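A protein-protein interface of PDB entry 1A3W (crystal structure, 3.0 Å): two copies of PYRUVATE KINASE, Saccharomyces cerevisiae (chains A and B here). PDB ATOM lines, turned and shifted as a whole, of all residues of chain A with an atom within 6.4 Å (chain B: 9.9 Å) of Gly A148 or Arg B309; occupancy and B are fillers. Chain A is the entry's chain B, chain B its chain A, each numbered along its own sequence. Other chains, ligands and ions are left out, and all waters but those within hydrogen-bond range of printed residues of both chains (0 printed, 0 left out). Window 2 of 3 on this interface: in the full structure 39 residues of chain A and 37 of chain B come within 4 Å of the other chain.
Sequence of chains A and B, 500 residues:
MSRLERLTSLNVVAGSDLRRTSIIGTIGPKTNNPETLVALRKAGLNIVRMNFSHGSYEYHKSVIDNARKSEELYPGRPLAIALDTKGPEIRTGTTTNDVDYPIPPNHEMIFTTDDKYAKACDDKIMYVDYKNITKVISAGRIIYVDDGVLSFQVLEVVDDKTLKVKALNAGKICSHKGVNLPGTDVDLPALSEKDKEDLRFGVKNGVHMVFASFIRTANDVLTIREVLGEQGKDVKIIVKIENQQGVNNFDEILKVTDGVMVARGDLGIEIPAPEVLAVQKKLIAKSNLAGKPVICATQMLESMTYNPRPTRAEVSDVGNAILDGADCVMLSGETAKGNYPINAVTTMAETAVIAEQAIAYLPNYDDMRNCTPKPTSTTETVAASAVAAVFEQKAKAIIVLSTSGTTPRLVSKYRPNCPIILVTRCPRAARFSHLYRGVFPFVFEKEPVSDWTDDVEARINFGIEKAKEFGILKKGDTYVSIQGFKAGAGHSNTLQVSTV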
ATOM      1  N   TYR A 144      14.559  -5.693  -6.614  1.00  0.00           N
ATOM      2  CA  TYR A 144      13.466  -6.169  -7.448  1.00  0.00           C
ATOM      3  C   TYR A 144      13.894  -7.443  -8.164  1.00  0.00           C
ATOM      4  O   TYR A 144      15.060  -7.605  -8.521  1.00  0.00           O
ATOM      5  CB  TYR A 144      13.075  -5.101  -8.466  1.00  0.00           C
ATOM      6  CG  TYR A 144      12.311  -3.960  -7.848  1.00  0.00           C
ATOM      7  CD1 TYR A 144      12.961  -3.016  -7.055  1.00  0.00           C
ATOM      8  CD2 TYR A 144      10.933  -3.843  -8.022  1.00  0.00           C
ATOM      9  CE1 TYR A 144      12.259  -1.985  -6.446  1.00  0.00           C
ATOM     10  CE2 TYR A 144      10.220  -2.815  -7.416  1.00  0.00           C
ATOM     11  CZ  TYR A 144      10.890  -1.890  -6.626  1.00  0.00           C
ATOM     12  OH  TYR A 144      10.193  -0.880  -6.002  1.00  0.00           O
ATOM     13  N   VAL A 145      12.943  -8.347  -8.362  1.00  0.00           N
ATOM     14  CA  VAL A 145      13.219  -9.610  -9.030  1.00  0.00           C
ATOM     15  C   VAL A 145      12.170  -9.890 -10.100  1.00  0.00           C
ATOM     16  O   VAL A 145      10.971  -9.791  -9.845  1.00  0.00           O
ATOM     17  CB  VAL A 145      13.232 -10.784  -8.022  1.00  0.00           C
ATOM     18  CG1 VAL A 145      13.270 -12.113  -8.759  1.00  0.00           C
ATOM     19  CG2 VAL A 145      14.436 -10.658  -7.098  1.00  0.00           C
ATOM     20  N   ASP A 146      12.635 -10.233 -11.297  1.00  0.00           N
ATOM     21  CA  ASP A 146      11.750 -10.545 -12.413  1.00  0.00           C
ATOM     22  C   ASP A 146      10.873  -9.357 -12.808  1.00  0.00           C
ATOM     23  O   ASP A 146       9.868  -9.077 -12.154  1.00  0.00           O
ATOM     24  CB  ASP A 146      10.871 -11.746 -12.048  1.00  0.00           C
ATOM     25  CG  ASP A 146       9.772 -12.002 -13.060  1.00  0.00           C
ATOM     26  OD1 ASP A 146       8.691 -11.386 -12.935  1.00  0.00           O
ATOM     27  OD2 ASP A 146       9.987 -12.820 -13.978  1.00  0.00           O
ATOM     28  N   ASP A 147      11.266  -8.666 -13.877  1.00  0.00           N
ATOM     29  CA  ASP A 147      10.517  -7.513 -14.378  1.00  0.00           C
ATOM     30  C   ASP A 147      10.233  -6.504 -13.268  1.00  0.00           C
ATOM     31  O   ASP A 147       9.337  -5.668 -13.386  1.00  0.00           O
ATOM     32  CB  ASP A 147       9.196  -7.990 -15.001  1.00  0.00           C
ATOM     33  CG  ASP A 147       8.428  -6.872 -15.687  1.00  0.00           C
ATOM     34  OD1 ASP A 147       8.991  -5.767 -15.852  1.00  0.00           O
ATOM     35  OD2 ASP A 147       7.258  -7.103 -16.063  1.00  0.00           O
ATOM     36  N   GLY A 148      11.005  -6.583 -12.189  1.00  0.00           N
ATOM     37  CA  GLY A 148      10.807  -5.677 -11.072  1.00  0.00           C
ATOM     38  C   GLY A 148       9.449  -5.897 -10.439  1.00  0.00           C
ATOM     39  O   GLY A 148       8.657  -4.966 -10.308  1.00  0.00           O
ATOM     40  N   VAL A 149       9.180  -7.139 -10.049  1.00  0.00           N
ATOM     41  CA  VAL A 149       7.906  -7.495  -9.430  1.00  0.00           C
ATOM     42  C   VAL A 149       8.067  -7.678  -7.925  1.00  0.00           C
ATOM     43  O   VAL A 149       7.429  -6.987  -7.129  1.00  0.00           O
ATOM     44  CB  VAL A 149       7.344  -8.807 -10.024  1.00  0.00           C
ATOM     45  CG1 VAL A 149       6.177  -9.302  -9.183  1.00  0.00           C
ATOM     46  CG2 VAL A 149       6.908  -8.584 -11.458  1.00  0.00           C
ATOM     47  N   LEU A 150       8.923  -8.616  -7.542  1.00  0.00           N
ATOM     48  CA  LEU A 150       9.170  -8.894  -6.140  1.00  0.00           C
ATOM     49  C   LEU A 150      10.131  -7.885  -5.528  1.00  0.00           C
ATOM     50  O   LEU A 150      11.270  -7.752  -5.970  1.00  0.00           O
ATOM     51  CB  LEU A 150       9.740 -10.299  -5.983  1.00  0.00           C
ATOM     52  CG  LEU A 150       8.673 -11.367  -5.754  1.00  0.00           C
ATOM     53  CD1 LEU A 150       8.400 -12.111  -7.055  1.00  0.00           C
ATOM     54  CD2 LEU A 150       9.136 -12.318  -4.665  1.00  0.00           C
ATOM     55  N   SER A 151       9.662  -7.174  -4.509  1.00  0.00           N
ATOM     56  CA  SER A 151      10.489  -6.188  -3.833  1.00  0.00           C
ATOM     57  C   SER A 151      10.980  -6.758  -2.508  1.00  0.00           C
ATOM     58  O   SER A 151      10.190  -7.208  -1.680  1.00  0.00           O
ATOM     59  CB  SER A 151       9.697  -4.900  -3.586  1.00  0.00           C
ATOM     60  OG  SER A 151       8.408  -4.959  -4.174  1.00  0.00           O
ATOM     61  N   GLY A 178      15.784 -11.941 -13.377  1.00  0.00           N
ATOM     62  CA  GLY A 178      16.669 -10.810 -13.171  1.00  0.00           C
ATOM     63  C   GLY A 178      16.618 -10.265 -11.757  1.00  0.00           C
ATOM     64  O   GLY A 178      15.566 -10.249 -11.123  1.00  0.00           O
ATOM     65  N   ASN A 180      17.280  -6.920 -10.064  1.00  0.00           N
ATOM     66  CA  ASN A 180      17.539  -5.492 -10.147  1.00  0.00           C
ATOM     67  C   ASN A 180      17.663  -4.892  -8.747  1.00  0.00           C
ATOM     68  O   ASN A 180      16.727  -4.955  -7.951  1.00  0.00           O
ATOM     69  CB  ASN A 180      16.404  -4.812 -10.909  1.00  0.00           C
ATOM     70  CG  ASN A 180      16.863  -4.214 -12.224  1.00  0.00           C
ATOM     71  OD1 ASN A 180      17.677  -3.291 -12.244  1.00  0.00           O
ATOM     72  ND2 ASN A 180      16.343  -4.736 -13.330  1.00  0.00           N
ATOM     73  N   GLY A 265      12.874  -0.618 -20.323  1.00  0.00           N
ATOM     74  CA  GLY A 265      12.715  -1.861 -19.578  1.00  0.00           C
ATOM     75  C   GLY A 265      13.369  -1.957 -18.207  1.00  0.00           C
ATOM     76  O   GLY A 265      12.697  -2.183 -17.201  1.00  0.00           O
ATOM     77  N   GLY A 268      13.049   1.804 -16.069  1.00  0.00           N
ATOM     78  CA  GLY A 268      11.888   1.907 -15.204  1.00  0.00           C
ATOM     79  C   GLY A 268      12.017   1.104 -13.927  1.00  0.00           C
ATOM     80  O   GLY A 268      11.205   1.231 -13.016  1.00  0.00           O
ATOM     81  N   ILE A 269      13.032   0.257 -13.858  1.00  0.00           N
ATOM     82  CA  ILE A 269      13.248  -0.534 -12.663  1.00  0.00           C
ATOM     83  C   ILE A 269      14.240   0.213 -11.784  1.00  0.00           C
ATOM     84  O   ILE A 269      14.063   0.302 -10.574  1.00  0.00           O
ATOM     85  CB  ILE A 269      13.818  -1.927 -12.999  1.00  0.00           C
ATOM     86  CG1 ILE A 269      13.044  -2.545 -14.164  1.00  0.00           C
ATOM     87  CG2 ILE A 269      13.738  -2.826 -11.772  1.00  0.00           C
ATOM     88  CD1 ILE A 269      11.668  -3.060 -13.784  1.00  0.00           C
ATOM     89  N   ILE A 271      15.192   3.643 -11.957  1.00  0.00           N
ATOM     90  CA  ILE A 271      14.598   4.902 -11.528  1.00  0.00           C
ATOM     91  C   ILE A 271      13.091   4.711 -11.547  1.00  0.00           C
ATOM     92  O   ILE A 271      12.575   3.946 -12.364  1.00  0.00           O
ATOM     93  CB  ILE A 271      14.961   6.064 -12.475  1.00  0.00           C
ATOM     94  CG1 ILE A 271      14.659   5.677 -13.927  1.00  0.00           C
ATOM     95  CG2 ILE A 271      16.427   6.430 -12.310  1.00  0.00           C
ATOM     96  CD1 ILE A 271      13.484   6.419 -14.533  1.00  0.00           C
ATOM     97  N   ALA A 273       9.511   4.319 -12.349  1.00  0.00           N
ATOM     98  CA  ALA A 273       8.846   4.231 -13.646  1.00  0.00           C
ATOM     99  C   ALA A 273       8.320   5.552 -14.215  1.00  0.00           C
ATOM    100  O   ALA A 273       8.516   5.849 -15.391  1.00  0.00           O
ATOM    101  CB  ALA A 273       7.709   3.216 -13.569  1.00  0.00           C
ATOM    102  N   MET B 300      -5.294   3.286 -20.587  1.00  0.00           N
ATOM    103  CA  MET B 300      -4.209   4.173 -20.183  1.00  0.00           C
ATOM    104  C   MET B 300      -3.251   3.427 -19.266  1.00  0.00           C
ATOM    105  O   MET B 300      -2.156   3.906 -18.962  1.00  0.00           O
ATOM    106  CB  MET B 300      -4.770   5.401 -19.465  1.00  0.00           C
ATOM    107  CG  MET B 300      -5.626   6.288 -20.349  1.00  0.00           C
ATOM    108  SD  MET B 300      -5.349   8.027 -20.021  1.00  0.00           S
ATOM    109  CE  MET B 300      -3.703   8.253 -20.717  1.00  0.00           C
ATOM    110  N   LEU B 301      -3.683   2.251 -18.825  1.00  0.00           N
ATOM    111  CA  LEU B 301      -2.885   1.405 -17.950  1.00  0.00           C
ATOM    112  C   LEU B 301      -3.534   0.025 -17.902  1.00  0.00           C
ATOM    113  O   LEU B 301      -3.636  -0.599 -16.842  1.00  0.00           O
ATOM    114  CB  LEU B 301      -2.807   2.006 -16.543  1.00  0.00           C
ATOM    115  CG  LEU B 301      -1.683   3.020 -16.283  1.00  0.00           C
ATOM    116  CD1 LEU B 301      -1.752   3.518 -14.849  1.00  0.00           C
ATOM    117  CD2 LEU B 301      -0.343   2.383 -16.546  1.00  0.00           C
ATOM    118  N   GLU B 302      -3.973  -0.439 -19.067  1.00  0.00           N
ATOM    119  CA  GLU B 302      -4.619  -1.738 -19.193  1.00  0.00           C
ATOM    120  C   GLU B 302      -3.835  -2.845 -18.501  1.00  0.00           C
ATOM    121  O   GLU B 302      -4.413  -3.687 -17.822  1.00  0.00           O
ATOM    122  CB  GLU B 302      -4.804  -2.094 -20.670  1.00  0.00           C
ATOM    123  CG  GLU B 302      -5.833  -3.188 -20.915  1.00  0.00           C
ATOM    124  CD  GLU B 302      -7.134  -2.941 -20.173  1.00  0.00           C
ATOM    125  OE1 GLU B 302      -7.172  -3.179 -18.947  1.00  0.00           O
ATOM    126  OE2 GLU B 302      -8.118  -2.510 -20.816  1.00  0.00           O
ATOM    127  N   SER B 303      -2.519  -2.845 -18.678  1.00  0.00           N
ATOM    128  CA  SER B 303      -1.680  -3.864 -18.063  1.00  0.00           C
ATOM    129  C   SER B 303      -1.868  -3.916 -16.544  1.00  0.00           C
ATOM    130  O   SER B 303      -1.885  -4.999 -15.953  1.00  0.00           O
ATOM    131  CB  SER B 303      -0.207  -3.608 -18.400  1.00  0.00           C
ATOM    132  OG  SER B 303       0.556  -3.300 -17.243  1.00  0.00           O
ATOM    133  N   MET B 304      -2.017  -2.750 -15.919  1.00  0.00           N
ATOM    134  CA  MET B 304      -2.200  -2.673 -14.470  1.00  0.00           C
ATOM    135  C   MET B 304      -3.463  -3.397 -14.034  1.00  0.00           C
ATOM    136  O   MET B 304      -3.691  -3.585 -12.840  1.00  0.00           O
ATOM    137  CB  MET B 304      -2.276  -1.219 -14.009  1.00  0.00           C
ATOM    138  CG  MET B 304      -1.124  -0.364 -14.486  1.00  0.00           C
ATOM    139  SD  MET B 304      -0.503   0.739 -13.212  1.00  0.00           S
ATOM    140  CE  MET B 304       0.473  -0.391 -12.227  1.00  0.00           C
ATOM    141  N   THR B 305      -4.279  -3.792 -15.008  1.00  0.00           N
ATOM    142  CA  THR B 305      -5.519  -4.508 -14.735  1.00  0.00           C
ATOM    143  C   THR B 305      -5.198  -5.901 -14.189  1.00  0.00           C
ATOM    144  O   THR B 305      -6.025  -6.522 -13.523  1.00  0.00           O
ATOM    145  CB  THR B 305      -6.385  -4.633 -16.018  1.00  0.00           C
ATOM    146  OG1 THR B 305      -7.767  -4.738 -15.661  1.00  0.00           O
ATOM    147  CG2 THR B 305      -5.983  -5.855 -16.826  1.00  0.00           C
ATOM    148  N   TYR B 306      -3.987  -6.381 -14.474  1.00  0.00           N
ATOM    149  CA  TYR B 306      -3.538  -7.691 -14.011  1.00  0.00           C
ATOM    150  C   TYR B 306      -2.094  -7.621 -13.525  1.00  0.00           C
ATOM    151  O   TYR B 306      -1.410  -8.639 -13.455  1.00  0.00           O
ATOM    152  CB  TYR B 306      -3.623  -8.718 -15.138  1.00  0.00           C
ATOM    153  CG  TYR B 306      -5.020  -9.001 -15.626  1.00  0.00           C
ATOM    154  CD1 TYR B 306      -6.046  -9.297 -14.731  1.00  0.00           C
ATOM    155  CD2 TYR B 306      -5.316  -8.982 -16.989  1.00  0.00           C
ATOM    156  CE1 TYR B 306      -7.337  -9.569 -15.181  1.00  0.00           C
ATOM    157  CE2 TYR B 306      -6.602  -9.251 -17.452  1.00  0.00           C
ATOM    158  CZ  TYR B 306      -7.607  -9.543 -16.542  1.00  0.00           C
ATOM    159  OH  TYR B 306      -8.881  -9.804 -16.993  1.00  0.00           O
ATOM    160  N   ASN B 307      -1.625  -6.423 -13.190  1.00  0.00           N
ATOM    161  CA  ASN B 307      -0.248  -6.264 -12.733  1.00  0.00           C
ATOM    162  C   ASN B 307      -0.039  -4.987 -11.923  1.00  0.00           C
ATOM    163  O   ASN B 307      -0.667  -3.961 -12.188  1.00  0.00           O
ATOM    164  CB  ASN B 307       0.695  -6.252 -13.938  1.00  0.00           C
ATOM    165  CG  ASN B 307       1.769  -7.313 -13.849  1.00  0.00           C
ATOM    166  OD1 ASN B 307       1.633  -8.395 -14.417  1.00  0.00           O
ATOM    167  ND2 ASN B 307       2.846  -7.007 -13.137  1.00  0.00           N
ATOM    168  N   PRO B 308       0.846  -5.041 -10.913  1.00  0.00           N
ATOM    169  CA  PRO B 308       1.139  -3.881 -10.067  1.00  0.00           C
ATOM    170  C   PRO B 308       2.183  -2.987 -10.728  1.00  0.00           C
ATOM    171  O   PRO B 308       2.509  -1.906 -10.228  1.00  0.00           O
ATOM    172  CB  PRO B 308       1.661  -4.509  -8.784  1.00  0.00           C
ATOM    173  CG  PRO B 308       2.331  -5.767  -9.247  1.00  0.00           C
ATOM    174  CD  PRO B 308       1.616  -6.227 -10.499  1.00  0.00           C
ATOM    175  N   ARG B 309       2.699  -3.457 -11.861  1.00  0.00           N
ATOM    176  CA  ARG B 309       3.711  -2.737 -12.624  1.00  0.00           C
ATOM    177  C   ARG B 309       3.223  -2.446 -14.040  1.00  0.00           C
ATOM    178  O   ARG B 309       2.877  -3.358 -14.794  1.00  0.00           O
ATOM    179  CB  ARG B 309       5.003  -3.557 -12.693  1.00  0.00           C
ATOM    180  CG  ARG B 309       5.746  -3.670 -11.374  1.00  0.00           C
ATOM    181  CD  ARG B 309       6.285  -2.322 -10.930  1.00  0.00           C
ATOM    182  NE  ARG B 309       7.649  -2.092 -11.401  1.00  0.00           N
ATOM    183  CZ  ARG B 309       7.955  -1.553 -12.578  1.00  0.00           C
ATOM    184  NH1 ARG B 309       6.993  -1.184 -13.415  1.00  0.00           N
ATOM    185  NH2 ARG B 309       9.227  -1.376 -12.914  1.00  0.00           N
ATOM    186  N   PRO B 310       3.192  -1.161 -14.420  1.00  0.00           N
ATOM    187  CA  PRO B 310       2.748  -0.740 -15.751  1.00  0.00           C
ATOM    188  C   PRO B 310       3.904  -0.772 -16.747  1.00  0.00           C
ATOM    189  O   PRO B 310       5.062  -0.581 -16.368  1.00  0.00           O
ATOM    190  CB  PRO B 310       2.249   0.677 -15.516  1.00  0.00           C
ATOM    191  CG  PRO B 310       3.143   1.191 -14.421  1.00  0.00           C
ATOM    192  CD  PRO B 310       3.575  -0.006 -13.587  1.00  0.00           C
ATOM    193  N   THR B 311       3.590  -1.009 -18.018  1.00  0.00           N
ATOM    194  CA  THR B 311       4.620  -1.050 -19.050  1.00  0.00           C
ATOM    195  C   THR B 311       5.079   0.356 -19.432  1.00  0.00           C
ATOM    196  O   THR B 311       4.331   1.323 -19.288  1.00  0.00           O
ATOM    197  CB  THR B 311       4.117  -1.764 -20.309  1.00  0.00           C
ATOM    198  OG1 THR B 311       3.084  -0.988 -20.922  1.00  0.00           O
ATOM    199  CG2 THR B 311       3.572  -3.133 -19.955  1.00  0.00           C
ATOM    200  N   ARG B 312       6.314   0.458 -19.916  1.00  0.00           N
ATOM    201  CA  ARG B 312       6.888   1.740 -20.316  1.00  0.00           C
ATOM    202  C   ARG B 312       5.938   2.541 -21.192  1.00  0.00           C
ATOM    203  O   ARG B 312       5.781   3.748 -21.011  1.00  0.00           O
ATOM    204  CB  ARG B 312       8.202   1.525 -21.075  1.00  0.00           C
ATOM    205  CG  ARG B 312       9.033   0.358 -20.583  1.00  0.00           C
ATOM    206  CD  ARG B 312       9.383   0.499 -19.108  1.00  0.00           C
ATOM    207  NE  ARG B 312       8.982  -0.683 -18.349  1.00  0.00           N
ATOM    208  CZ  ARG B 312       9.571  -1.090 -17.230  1.00  0.00           C
ATOM    209  NH1 ARG B 312      10.597  -0.406 -16.731  1.00  0.00           N
ATOM    210  NH2 ARG B 312       9.142  -2.186 -16.612  1.00  0.00           N
ATOM    211  N   ALA B 313       5.309   1.858 -22.144  1.00  0.00           N
ATOM    212  CA  ALA B 313       4.375   2.494 -23.065  1.00  0.00           C
ATOM    213  C   ALA B 313       3.173   3.067 -22.328  1.00  0.00           C
ATOM    214  O   ALA B 313       2.627   4.099 -22.719  1.00  0.00           O
ATOM    215  CB  ALA B 313       3.908   1.488 -24.108  1.00  0.00           C
ATOM    216  N   GLU B 314       2.768   2.392 -21.259  1.00  0.00           N
ATOM    217  CA  GLU B 314       1.621   2.819 -20.475  1.00  0.00           C
ATOM    218  C   GLU B 314       1.819   4.167 -19.804  1.00  0.00           C
ATOM    219  O   GLU B 314       1.073   5.107 -20.076  1.00  0.00           O
ATOM    220  CB  GLU B 314       1.289   1.762 -19.430  1.00  0.00           C
ATOM    221  CG  GLU B 314      -0.064   1.119 -19.653  1.00  0.00           C
ATOM    222  CD  GLU B 314      -0.029  -0.381 -19.509  1.00  0.00           C
ATOM    223  OE1 GLU B 314       0.727  -0.870 -18.640  1.00  0.00           O
ATOM    224  OE2 GLU B 314      -0.760  -1.066 -20.263  1.00  0.00           O
ATOM    225  N   VAL B 315       2.812   4.264 -18.925  1.00  0.00           N
ATOM    226  CA  VAL B 315       3.072   5.528 -18.241  1.00  0.00           C
ATOM    227  C   VAL B 315       3.286   6.628 -19.279  1.00  0.00           C
ATOM    228  O   VAL B 315       2.841   7.762 -19.099  1.00  0.00           O
ATOM    229  CB  VAL B 315       4.306   5.437 -17.288  1.00  0.00           C
ATOM    230  CG1 VAL B 315       5.096   4.181 -17.568  1.00  0.00           C
ATOM    231  CG2 VAL B 315       5.185   6.661 -17.439  1.00  0.00           C
ATOM    232  N   ASN B 339      -7.050  -6.384 -10.761  1.00  0.00           N
ATOM    233  CA  ASN B 339      -6.523  -6.940  -9.524  1.00  0.00           C
ATOM    234  C   ASN B 339      -5.574  -5.965  -8.834  1.00  0.00           C
ATOM    235  O   ASN B 339      -4.950  -6.298  -7.829  1.00  0.00           O
ATOM    236  CB  ASN B 339      -5.792  -8.251  -9.814  1.00  0.00           C
ATOM    237  CG  ASN B 339      -6.428  -9.436  -9.117  1.00  0.00           C
ATOM    238  OD1 ASN B 339      -5.773 -10.148  -8.355  1.00  0.00           O
ATOM    239  ND2 ASN B 339      -7.712  -9.653  -9.375  1.00  0.00           N
ATOM    240  N   TYR B 340      -5.463  -4.762  -9.385  1.00  0.00           N
ATOM    241  CA  TYR B 340      -4.598  -3.735  -8.819  1.00  0.00           C
ATOM    242  C   TYR B 340      -5.196  -2.367  -9.114  1.00  0.00           C
ATOM    243  O   TYR B 340      -4.755  -1.672 -10.027  1.00  0.00           O
ATOM    244  CB  TYR B 340      -3.194  -3.830  -9.420  1.00  0.00           C
ATOM    245  CG  TYR B 340      -2.474  -5.124  -9.108  1.00  0.00           C
ATOM    246  CD1 TYR B 340      -1.879  -5.333  -7.864  1.00  0.00           C
ATOM    247  CD2 TYR B 340      -2.390  -6.143 -10.056  1.00  0.00           C
ATOM    248  CE1 TYR B 340      -1.218  -6.527  -7.573  1.00  0.00           C
ATOM    249  CE2 TYR B 340      -1.730  -7.340  -9.776  1.00  0.00           C
ATOM    250  CZ  TYR B 340      -1.148  -7.527  -8.535  1.00  0.00           C
ATOM    251  OH  TYR B 340      -0.503  -8.712  -8.259  1.00  0.00           O
ATOM    252  N   PRO B 341      -6.222  -1.967  -8.344  1.00  0.00           N
ATOM    253  CA  PRO B 341      -6.888  -0.673  -8.528  1.00  0.00           C
ATOM    254  C   PRO B 341      -6.119   0.508  -7.950  1.00  0.00           C
ATOM    255  O   PRO B 341      -5.650   1.372  -8.687  1.00  0.00           O
ATOM    256  CB  PRO B 341      -8.235  -0.868  -7.843  1.00  0.00           C
ATOM    257  CG  PRO B 341      -7.956  -1.860  -6.767  1.00  0.00           C
ATOM    258  CD  PRO B 341      -6.823  -2.740  -7.241  1.00  0.00           C
ATOM    259  N   ASN B 343      -3.255   0.733  -6.932  1.00  0.00           N
ATOM    260  CA  ASN B 343      -1.920   0.782  -7.516  1.00  0.00           C
ATOM    261  C   ASN B 343      -1.949   1.518  -8.857  1.00  0.00           C
ATOM    262  O   ASN B 343      -1.081   2.347  -9.140  1.00  0.00           O
ATOM    263  CB  ASN B 343      -1.384  -0.642  -7.698  1.00  0.00           C
ATOM    264  CG  ASN B 343      -1.778  -1.563  -6.548  1.00  0.00           C
ATOM    265  OD1 ASN B 343      -2.825  -2.220  -6.590  1.00  0.00           O
ATOM    266  ND2 ASN B 343      -0.943  -1.607  -5.510  1.00  0.00           N
ATOM    267  N   ALA B 344      -2.951   1.210  -9.676  1.00  0.00           N
ATOM    268  CA  ALA B 344      -3.099   1.855 -10.976  1.00  0.00           C
ATOM    269  C   ALA B 344      -3.210   3.360 -10.758  1.00  0.00           C
ATOM    270  O   ALA B 344      -2.390   4.136 -11.261  1.00  0.00           O
ATOM    271  CB  ALA B 344      -4.343   1.342 -11.679  1.00  0.00           C
ATOM    272  N   THR B 347       0.011   5.004  -9.720  1.00  0.00           N
ATOM    273  CA  THR B 347       0.929   5.114 -10.848  1.00  0.00           C
ATOM    274  C   THR B 347       0.542   6.260 -11.766  1.00  0.00           C
ATOM    275  O   THR B 347       1.407   6.942 -12.322  1.00  0.00           O
ATOM    276  CB  THR B 347       0.954   3.836 -11.673  1.00  0.00           C
ATOM    277  OG1 THR B 347       1.279   2.731 -10.826  1.00  0.00           O
ATOM    278  CG2 THR B 347       1.988   3.951 -12.777  1.00  0.00           C
ATOM    279  N   GLU B 350       1.286   9.736  -9.973  1.00  0.00           N
ATOM    280  CA  GLU B 350       2.731   9.935  -9.970  1.00  0.00           C
ATOM    281  C   GLU B 350       3.221  10.361 -11.346  1.00  0.00           C
ATOM    282  O   GLU B 350       4.067  11.247 -11.472  1.00  0.00           O
ATOM    283  CB  GLU B 350       3.437   8.648  -9.543  1.00  0.00           C
ATOM    284  CG  GLU B 350       4.045   8.706  -8.150  1.00  0.00           C
ATOM    285  CD  GLU B 350       4.282   7.328  -7.566  1.00  0.00           C
ATOM    286  OE1 GLU B 350       4.199   6.340  -8.327  1.00  0.00           O
ATOM    287  OE2 GLU B 350       4.551   7.232  -6.351  1.00  0.00           O
ATOM    288  N   THR B 351       2.682   9.717 -12.374  1.00  0.00           N
ATOM    289  CA  THR B 351       3.050  10.029 -13.745  1.00  0.00           C
ATOM    290  C   THR B 351       2.570  11.432 -14.079  1.00  0.00           C
ATOM    291  O   THR B 351       3.270  12.201 -14.739  1.00  0.00           O
ATOM    292  CB  THR B 351       2.402   9.048 -14.726  1.00  0.00           C
ATOM    293  OG1 THR B 351       2.846   7.718 -14.434  1.00  0.00           O
ATOM    294  CG2 THR B 351       2.767   9.412 -16.156  1.00  0.00           C
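The backbone carbonyl oxygen (O) of Gly A148 lies within hydrogen-bond range of the guanidinium group (NE) of Arg B309 (3.2 Å).
The backbone carbonyl oxygen (O) of Gly A268 lies within hydrogen-bond range of the guanidinium group (NH2) of Arg B309 (3.3 Å).
The guanidinium group (NH2) of Arg B312 is in salt-bridge range of the side-chain carboxylate (OD1) of Asp A147.
The backbone carbonyl oxygen (O) of Gly A265 is in hydrogen-bond range of the guanidinium group (NH1) of Arg B312, 2.8 Å away.
The backbone NH of Gly A268 sits close to the guanidinium group of Arg B312, 3.4 Å away.
OG of Ser B303 lies within hydrogen-bond range of O of Arg B309 (3.4 Å).
Among the printed residues, merely in contact across the chains: Ile A269 with Arg B309, Ile A269 with Arg B312 and Ala A273 with Val B315.
Of chain B, only Arg B309 comes within 4 Å of Gly A148.
Of chain A, only Gly A148, Gly A268 and Ile A269 come within 4 Å of Arg B309.
Ile A269 touches just these residues of chain B: Arg B309 (3.1 Å) and Arg B312 (3.8 Å).
Printed residues of chain B within 4 Å of Gly A268: Arg B309 and Arg B312.
Printed residues of chain B within 4 Å of Ala A273: Val B315.
The nearest residue of chain B that does not touch Gly A148 is Pro B308 (6.5 Å).
The nearest residue of chain A that does not touch Arg B309 is Asp A147 (4.3 Å).
The nearest printed residue of chain B that does not touch Gly A265 is Arg B309 (5.6 Å).
Printed residues of chain B that touch a printed residue of chain A: Arg B309, Arg B312 and Val B315.
Hydrophobic or aromatic side chains of chain B within 4 Å of the printed part of chain A: Val B315.
Of the 15 printed residues of chain A, 6 touch a printed residue of chain B.
No position is printed for both chains.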
